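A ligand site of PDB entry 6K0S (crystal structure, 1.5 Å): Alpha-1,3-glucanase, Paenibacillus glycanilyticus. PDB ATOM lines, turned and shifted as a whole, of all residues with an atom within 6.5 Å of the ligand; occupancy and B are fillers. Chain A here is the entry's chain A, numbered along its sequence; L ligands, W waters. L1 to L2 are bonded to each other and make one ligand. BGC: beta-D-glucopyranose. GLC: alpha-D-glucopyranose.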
ATOM      1  N   THR A  86      34.108 -35.136 -12.242  1.00  0.00           N
ATOM      2  CA  THR A  86      33.262 -33.978 -12.000  1.00  0.00           C
ATOM      3  C   THR A  86      32.865 -33.411 -13.344  1.00  0.00           C
ATOM      4  O   THR A  86      33.547 -33.601 -14.353  1.00  0.00           O
ATOM      5  CB  THR A  86      33.950 -32.888 -11.181  1.00  0.00           C
ATOM      6  OG1 THR A  86      35.026 -32.335 -11.953  1.00  0.00           O
ATOM      7  CG2 THR A  86      34.482 -33.436  -9.848  1.00  0.00           C
ATOM      8  N   PHE A 101      23.973 -28.006 -13.410  1.00  0.00           N
ATOM      9  CA  PHE A 101      24.317 -28.634 -12.137  1.00  0.00           C
ATOM     10  C   PHE A 101      25.790 -28.997 -12.130  1.00  0.00           C
ATOM     11  O   PHE A 101      26.330 -29.451 -13.135  1.00  0.00           O
ATOM     12  CB  PHE A 101      23.513 -29.922 -11.949  1.00  0.00           C
ATOM     13  CG  PHE A 101      22.069 -29.712 -11.618  1.00  0.00           C
ATOM     14  CD1 PHE A 101      21.656 -29.555 -10.302  1.00  0.00           C
ATOM     15  CD2 PHE A 101      21.121 -29.713 -12.631  1.00  0.00           C
ATOM     16  CE1 PHE A 101      20.311 -29.386 -10.003  1.00  0.00           C
ATOM     17  CE2 PHE A 101      19.767 -29.546 -12.329  1.00  0.00           C
ATOM     18  CZ  PHE A 101      19.363 -29.387 -11.017  1.00  0.00           C
ATOM     19  N   ASN A 102      26.413 -28.869 -10.967  1.00  0.00           N
ATOM     20  CA  ASN A 102      27.764 -29.376 -10.720  1.00  0.00           C
ATOM     21  C   ASN A 102      27.607 -30.791 -10.180  1.00  0.00           C
ATOM     22  O   ASN A 102      27.251 -30.982  -9.012  1.00  0.00           O
ATOM     23  CB  ASN A 102      28.500 -28.462  -9.737  1.00  0.00           C
ATOM     24  CG  ASN A 102      29.925 -28.930  -9.438  1.00  0.00           C
ATOM     25  OD1 ASN A 102      30.208 -30.122  -9.349  1.00  0.00           O
ATOM     26  ND2 ASN A 102      30.818 -27.970  -9.262  1.00  0.00           N
ATOM     27  N   VAL A 103      27.857 -31.792 -11.027  1.00  0.00           N
ATOM     28  CA  VAL A 103      27.717 -33.190 -10.633  1.00  0.00           C
ATOM     29  C   VAL A 103      29.084 -33.794 -10.389  1.00  0.00           C
ATOM     30  O   VAL A 103      30.084 -33.425 -11.034  1.00  0.00           O
ATOM     31  CB  VAL A 103      26.920 -33.993 -11.693  1.00  0.00           C
ATOM     32  CG1 VAL A 103      25.494 -33.466 -11.772  1.00  0.00           C
ATOM     33  CG2 VAL A 103      27.602 -33.919 -13.055  1.00  0.00           C
ATOM     34  N   SER A 104      29.161 -34.726  -9.442  1.00  0.00           N
ATOM     35  CA  SER A 104      30.452 -35.240  -9.034  1.00  0.00           C
ATOM     36  C   SER A 104      30.268 -36.575  -8.325  1.00  0.00           C
ATOM     37  O   SER A 104      29.241 -36.813  -7.680  1.00  0.00           O
ATOM     38  CB  SER A 104      31.158 -34.250  -8.099  1.00  0.00           C
ATOM     39  OG  SER A 104      32.319 -34.823  -7.555  1.00  0.00           O
ATOM     40  N   LYS A 106      32.651 -37.337  -6.075  1.00  0.00           N
ATOM     41  CA  LYS A 106      33.601 -37.189  -4.973  1.00  0.00           C
ATOM     42  C   LYS A 106      33.165 -37.953  -3.727  1.00  0.00           C
ATOM     43  O   LYS A 106      33.986 -38.602  -3.056  1.00  0.00           O
ATOM     44  CB  LYS A 106      33.781 -35.710  -4.639  1.00  0.00           C
ATOM     45  CG  LYS A 106      34.551 -35.496  -3.345  1.00  0.00           C
ATOM     46  CD  LYS A 106      34.675 -34.009  -3.040  1.00  0.00           C
ATOM     47  CE  LYS A 106      35.534 -33.792  -1.801  1.00  0.00           C
ATOM     48  NZ  LYS A 106      35.857 -32.347  -1.616  1.00  0.00           N
ATOM     49  N   PHE A 107      31.867 -37.929  -3.419  1.00  0.00           N
ATOM     50  CA  PHE A 107      31.351 -38.515  -2.187  1.00  0.00           C
ATOM     51  C   PHE A 107      30.708 -39.883  -2.368  1.00  0.00           C
ATOM     52  O   PHE A 107      30.351 -40.517  -1.370  1.00  0.00           O
ATOM     53  CB  PHE A 107      30.344 -37.557  -1.530  1.00  0.00           C
ATOM     54  CG  PHE A 107      30.983 -36.301  -1.034  1.00  0.00           C
ATOM     55  CD1 PHE A 107      31.674 -36.317   0.164  1.00  0.00           C
ATOM     56  CD2 PHE A 107      30.927 -35.117  -1.760  1.00  0.00           C
ATOM     57  CE1 PHE A 107      32.294 -35.158   0.650  1.00  0.00           C
ATOM     58  CE2 PHE A 107      31.530 -33.954  -1.287  1.00  0.00           C
ATOM     59  CZ  PHE A 107      32.225 -33.974  -0.081  1.00  0.00           C
ATOM     60  N   ASP A 138      24.376 -36.180  -5.016  1.00  0.00           N
ATOM     61  CA  ASP A 138      23.430 -35.085  -5.233  1.00  0.00           C
ATOM     62  C   ASP A 138      24.139 -33.839  -5.765  1.00  0.00           C
ATOM     63  O   ASP A 138      25.279 -33.544  -5.394  1.00  0.00           O
ATOM     64  CB  ASP A 138      22.704 -34.682  -3.939  1.00  0.00           C
ATOM     65  CG  ASP A 138      21.773 -35.773  -3.406  1.00  0.00           C
ATOM     66  OD1 ASP A 138      21.570 -36.818  -4.078  1.00  0.00           O
ATOM     67  OD2 ASP A 138      21.229 -35.551  -2.297  1.00  0.00           O
ATOM     68  N   ALA A 139      23.410 -33.086  -6.581  1.00  0.00           N
ATOM     69  CA  ALA A 139      23.846 -31.770  -7.017  1.00  0.00           C
ATOM     70  C   ALA A 139      22.761 -30.756  -6.669  1.00  0.00           C
ATOM     71  O   ALA A 139      21.577 -31.017  -6.894  1.00  0.00           O
ATOM     72  CB  ALA A 139      24.142 -31.741  -8.528  1.00  0.00           C
ATOM     73  N   GLN A 140      23.158 -29.602  -6.131  1.00  0.00           N
ATOM     74  CA  GLN A 140      22.243 -28.571  -5.670  1.00  0.00           C
ATOM     75  C   GLN A 140      22.378 -27.334  -6.553  1.00  0.00           C
ATOM     76  O   GLN A 140      23.497 -26.920  -6.879  1.00  0.00           O
ATOM     77  CB  GLN A 140      22.528 -28.188  -4.210  1.00  0.00           C
ATOM     78  CG  GLN A 140      22.474 -29.354  -3.203  1.00  0.00           C
ATOM     79  CD  GLN A 140      23.707 -30.263  -3.255  1.00  0.00           C
ATOM     80  OE1 GLN A 140      24.817 -29.824  -3.588  1.00  0.00           O
ATOM     81  NE2 GLN A 140      23.513 -31.530  -2.933  1.00  0.00           N
ATOM     82  N   LEU A 141      21.242 -26.717  -6.910  1.00  0.00           N
ATOM     83  CA  LEU A 141      21.275 -25.587  -7.825  1.00  0.00           C
ATOM     84  C   LEU A 141      20.093 -24.674  -7.545  1.00  0.00           C
ATOM     85  O   LEU A 141      18.960 -25.137  -7.440  1.00  0.00           O
ATOM     86  CB  LEU A 141      21.230 -26.061  -9.277  1.00  0.00           C
ATOM     87  CG  LEU A 141      21.383 -24.968 -10.342  1.00  0.00           C
ATOM     88  CD1 LEU A 141      22.799 -24.456 -10.305  1.00  0.00           C
ATOM     89  CD2 LEU A 141      21.067 -25.534 -11.734  1.00  0.00           C
ATOM     90  N   MET A 142      20.372 -23.375  -7.414  1.00  0.00           N
ATOM     91  CA  MET A 142      19.317 -22.370  -7.314  1.00  0.00           C
ATOM     92  C   MET A 142      19.312 -21.522  -8.576  1.00  0.00           C
ATOM     93  O   MET A 142      20.370 -21.144  -9.091  1.00  0.00           O
ATOM     94  CB  MET A 142      19.516 -21.485  -6.072  1.00  0.00           C
ATOM     95  CG  MET A 142      18.429 -20.421  -5.894  1.00  0.00           C
ATOM     96  SD  MET A 142      18.320 -19.784  -4.195  1.00  0.00           S
ATOM     97  CE  MET A 142      19.671 -20.680  -3.456  1.00  0.00           C
ATOM     98  N   GLU A 218      29.496 -19.080   2.424  1.00  0.00           N
ATOM     99  CA  GLU A 218      30.217 -20.289   2.778  1.00  0.00           C
ATOM    100  C   GLU A 218      31.215 -19.941   3.871  1.00  0.00           C
ATOM    101  O   GLU A 218      32.026 -19.023   3.708  1.00  0.00           O
ATOM    102  CB  GLU A 218      30.950 -20.869   1.571  1.00  0.00           C
ATOM    103  CG  GLU A 218      30.044 -21.269   0.420  1.00  0.00           C
ATOM    104  CD  GLU A 218      30.820 -21.974  -0.684  1.00  0.00           C
ATOM    105  OE1 GLU A 218      31.976 -22.388  -0.440  1.00  0.00           O
ATOM    106  OE2 GLU A 218      30.262 -22.128  -1.782  1.00  0.00           O
ATOM    107  N   TRP A 240      19.570 -23.116   2.570  1.00  0.00           N
ATOM    108  CA  TRP A 240      20.093 -22.896   1.220  1.00  0.00           C
ATOM    109  C   TRP A 240      21.084 -21.758   1.147  1.00  0.00           C
ATOM    110  O   TRP A 240      21.756 -21.593   0.120  1.00  0.00           O
ATOM    111  CB  TRP A 240      18.951 -22.609   0.239  1.00  0.00           C
ATOM    112  CG  TRP A 240      18.291 -23.828  -0.338  1.00  0.00           C
ATOM    113  CD1 TRP A 240      17.192 -24.477   0.150  1.00  0.00           C
ATOM    114  CD2 TRP A 240      18.690 -24.541  -1.507  1.00  0.00           C
ATOM    115  NE1 TRP A 240      16.882 -25.549  -0.649  1.00  0.00           N
ATOM    116  CE2 TRP A 240      17.782 -25.603  -1.684  1.00  0.00           C
ATOM    117  CE3 TRP A 240      19.728 -24.372  -2.441  1.00  0.00           C
ATOM    118  CZ2 TRP A 240      17.882 -26.515  -2.740  1.00  0.00           C
ATOM    119  CZ3 TRP A 240      19.816 -25.283  -3.503  1.00  0.00           C
ATOM    120  CH2 TRP A 240      18.908 -26.331  -3.638  1.00  0.00           C
ATOM    121  N   LYS A 243      25.992 -21.697   4.674  1.00  0.00           N
ATOM    122  CA  LYS A 243      26.656 -22.982   4.468  1.00  0.00           C
ATOM    123  C   LYS A 243      27.917 -23.047   5.318  1.00  0.00           C
ATOM    124  O   LYS A 243      28.860 -22.285   5.091  1.00  0.00           O
ATOM    125  CB  LYS A 243      27.003 -23.191   2.994  1.00  0.00           C
ATOM    126  CG  LYS A 243      25.784 -23.141   2.068  1.00  0.00           C
ATOM    127  CD  LYS A 243      26.198 -23.182   0.610  1.00  0.00           C
ATOM    128  CE  LYS A 243      25.008 -22.962  -0.315  1.00  0.00           C
ATOM    129  NZ  LYS A 243      25.417 -23.158  -1.731  1.00  0.00           N
ATOM    130  N   VAL A 245      31.136 -25.126   5.948  1.00  0.00           N
ATOM    131  CA  VAL A 245      31.832 -25.978   4.989  1.00  0.00           C
ATOM    132  C   VAL A 245      33.115 -26.514   5.620  1.00  0.00           C
ATOM    133  O   VAL A 245      34.020 -25.731   5.952  1.00  0.00           O
ATOM    134  CB  VAL A 245      32.131 -25.242   3.680  1.00  0.00           C
ATOM    135  CG1 VAL A 245      32.807 -26.174   2.696  1.00  0.00           C
ATOM    136  CG2 VAL A 245      30.841 -24.686   3.074  1.00  0.00           C
ATOM    137  N   GLN A 248      37.309 -28.600   1.991  1.00  0.00           N
ATOM    138  CA  GLN A 248      37.004 -29.643   1.022  1.00  0.00           C
ATOM    139  C   GLN A 248      38.250 -30.240   0.366  1.00  0.00           C
ATOM    140  O   GLN A 248      38.136 -31.289  -0.280  1.00  0.00           O
ATOM    141  CB  GLN A 248      36.052 -29.100  -0.051  1.00  0.00           C
ATOM    142  CG  GLN A 248      34.632 -28.856   0.488  1.00  0.00           C
ATOM    143  CD  GLN A 248      33.992 -30.134   1.031  1.00  0.00           C
ATOM    144  OE1 GLN A 248      34.062 -31.172   0.381  1.00  0.00           O
ATOM    145  NE2 GLN A 248      33.401 -30.067   2.217  1.00  0.00           N
ATOM    146  N   TRP A 274      28.200 -28.823   5.431  1.00  0.00           N
ATOM    147  CA  TRP A 274      28.696 -29.617   4.310  1.00  0.00           C
ATOM    148  C   TRP A 274      30.025 -30.237   4.736  1.00  0.00           C
ATOM    149  O   TRP A 274      31.057 -29.571   4.699  1.00  0.00           O
ATOM    150  CB  TRP A 274      28.808 -28.730   3.066  1.00  0.00           C
ATOM    151  CG  TRP A 274      27.440 -28.307   2.621  1.00  0.00           C
ATOM    152  CD1 TRP A 274      26.754 -27.167   2.979  1.00  0.00           C
ATOM    153  CD2 TRP A 274      26.571 -29.044   1.773  1.00  0.00           C
ATOM    154  NE1 TRP A 274      25.516 -27.150   2.386  1.00  0.00           N
ATOM    155  CE2 TRP A 274      25.379 -28.294   1.636  1.00  0.00           C
ATOM    156  CE3 TRP A 274      26.682 -30.264   1.093  1.00  0.00           C
ATOM    157  CZ2 TRP A 274      24.308 -28.741   0.861  1.00  0.00           C
ATOM    158  CZ3 TRP A 274      25.623 -30.703   0.327  1.00  0.00           C
ATOM    159  CH2 TRP A 274      24.452 -29.944   0.221  1.00  0.00           C
ATOM    160  N   GLY A 275      29.973 -31.485   5.186  1.00  0.00           N
ATOM    161  CA  GLY A 275      31.162 -32.151   5.675  1.00  0.00           C
ATOM    162  C   GLY A 275      32.085 -32.558   4.545  1.00  0.00           C
ATOM    163  O   GLY A 275      31.812 -32.410   3.350  1.00  0.00           O
ATOM    164  N   HIS A 305      27.409 -35.447   4.424  1.00  0.00           N
ATOM    165  CA  HIS A 305      28.815 -35.851   4.339  1.00  0.00           C
ATOM    166  C   HIS A 305      29.526 -35.740   5.691  1.00  0.00           C
ATOM    167  O   HIS A 305      30.708 -35.388   5.777  1.00  0.00           O
ATOM    168  CB  HIS A 305      29.545 -35.064   3.244  1.00  0.00           C
ATOM    169  CG  HIS A 305      28.863 -35.172   1.915  1.00  0.00           C
ATOM    170  ND1 HIS A 305      28.774 -34.124   1.025  1.00  0.00           N
ATOM    171  CD2 HIS A 305      28.209 -36.213   1.342  1.00  0.00           C
ATOM    172  CE1 HIS A 305      28.096 -34.517  -0.046  1.00  0.00           C
ATOM    173  NE2 HIS A 305      27.741 -35.779   0.119  1.00  0.00           N
HETATM  174  C2  BGC L   1      29.692 -26.253  -3.376  1.00  0.00           C
HETATM  175  C3  BGC L   1      29.563 -26.835  -4.785  1.00  0.00           C
HETATM  176  C4  BGC L   1      28.132 -26.725  -5.288  1.00  0.00           C
HETATM  177  C5  BGC L   1      27.663 -25.286  -5.149  1.00  0.00           C
HETATM  178  C6  BGC L   1      26.269 -25.057  -5.727  1.00  0.00           C
HETATM  179  C1  BGC L   1      29.005 -24.884  -3.254  1.00  0.00           C
HETATM  180  O1  BGC L   1      28.947 -24.521  -1.894  1.00  0.00           O
HETATM  181  O2  BGC L   1      31.059 -26.130  -3.039  1.00  0.00           O
HETATM  182  O3  BGC L   1      29.965 -28.191  -4.744  1.00  0.00           O
HETATM  183  O4  BGC L   1      28.040 -27.150  -6.622  1.00  0.00           O
HETATM  184  O5  BGC L   1      27.696 -24.953  -3.777  1.00  0.00           O
HETATM  185  O6  BGC L   1      25.311 -25.784  -4.983  1.00  0.00           O
HETATM  186  C1  GLC L   2      31.098 -28.578  -5.418  1.00  0.00           C
HETATM  187  C2  GLC L   2      31.177 -30.085  -5.642  1.00  0.00           C
HETATM  188  C3  GLC L   2      31.515 -30.789  -4.329  1.00  0.00           C
HETATM  189  C4  GLC L   2      32.795 -30.204  -3.743  1.00  0.00           C
HETATM  190  C5  GLC L   2      32.663 -28.687  -3.621  1.00  0.00           C
HETATM  191  C6  GLC L   2      33.996 -28.112  -3.139  1.00  0.00           C
HETATM  192  O2  GLC L   2      29.969 -30.576  -6.198  1.00  0.00           O
HETATM  193  O3  GLC L   2      31.741 -32.166  -4.533  1.00  0.00           O
HETATM  194  O4  GLC L   2      33.070 -30.749  -2.472  1.00  0.00           O
HETATM  195  O5  GLC L   2      32.307 -28.096  -4.867  1.00  0.00           O
HETATM  196  O6  GLC L   2      34.986 -28.346  -4.131  1.00  0.00           O
HETATM  197  O   HOH W   1      36.563 -30.571  -3.648  1.00  0.00           O
HETATM  198  O   HOH W   2      32.672 -24.716  -4.800  1.00  0.00           O
HETATM  199  O   HOH W   3      26.686 -24.780  -9.070  1.00  0.00           O
HETATM  200  O   HOH W   4      35.381 -25.482  -5.031  1.00  0.00           O
HETATM  201  O   HOH W   5      30.711 -27.322   0.131  1.00  0.00           O
HETATM  202  O   HOH W   6      27.486 -30.235  -4.497  1.00  0.00           O
HETATM  203  O   HOH W   7      30.938 -30.159  -0.587  1.00  0.00           O
HETATM  204  O   HOH W   8      27.798 -21.511  -2.308  1.00  0.00           O
HETATM  205  O   HOH W   9      27.559 -32.637  -6.693  1.00  0.00           O
HETATM  206  O   HOH W  10      28.315 -26.611  -0.231  1.00  0.00           O
HETATM  207  O   HOH W  11      29.258 -33.594  -4.760  1.00  0.00           O
HETATM  208  O   HOH W  12      33.280 -27.465  -7.697  1.00  0.00           O
HETATM  209  O   HOH W  13      33.393 -32.470  -6.555  1.00  0.00           O
HETATM  210  O   HOH W  14      32.281 -25.227  -0.777  1.00  0.00           O
HETATM  211  O   HOH W  15      28.768 -30.018  -2.172  1.00  0.00           O
HETATM  212  O   HOH W  16      26.183 -29.301  -6.750  1.00  0.00           O
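The side-chain carboxylate (OE2) of Glu 218 lies within hydrogen-bond range of an oxygen (O1) of BGC L1. O6 of BGC L1 sits at hydrogen-bond distance from O of Gln 140 (2.9 Å). OE1 of Gln 248 lies within hydrogen-bond range of O4 of GLC L2, at 3.1 Å. OD1 of Asn 102 sits at hydrogen-bond distance from O2 of GLC L2 (3.2 Å). An oxygen (O4) of GLC L2 sits at hydrogen-bond distance from the side-chain amino group of Lys 106, at 3.3 Å.
NZ of Lys 106 sits at hydrogen-bond distance from O of Gln 248 (2.8 Å). The side-chain amide nitrogen (NE2) of Gln 248 is in hydrogen-bond range of the backbone carbonyl oxygen (O) of Trp 274, at 3.4 Å. NE2 of Gln 248 is in hydrogen-bond range of O of Gly 275, at 3.0 Å. OG of Ser 104 sits at hydrogen-bond distance from N of Lys 106 (2.9 Å).
CE2 of Phe 107 touches O3 of GLC L2 (3.7 Å). NZ of Lys 243 touches O5 of BGC L1 (3.5 Å). Seven residues have an atom within 4 Å of the ligand: Asn 102, Lys 106, Phe 107, Gln 140, Glu 218, Lys 243 and Gln 248. The nearest printed residue that does not touch the ligand is Ser 104 (4.1 Å).
Water W13 lies within hydrogen-bond range of O3 of GLC L2 and OG of Ser 104. Water W14 bridges O2 of BGC L1 and OE1 of Glu 218. Water W7 bridges O4 of GLC L2 and OE1 of Gln 248. Water W6 bridges OE1 of Gln 140 and O2 of GLC L2. Water W12 lies within hydrogen-bond range of ND2 of Asn 102 and O5 of GLC L2. Water W9 lies within hydrogen-bond range of the backbone carbonyl oxygen of Asp 138, the backbone carbonyl oxygen of Asn 102 and an oxygen (O2) of GLC L2.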
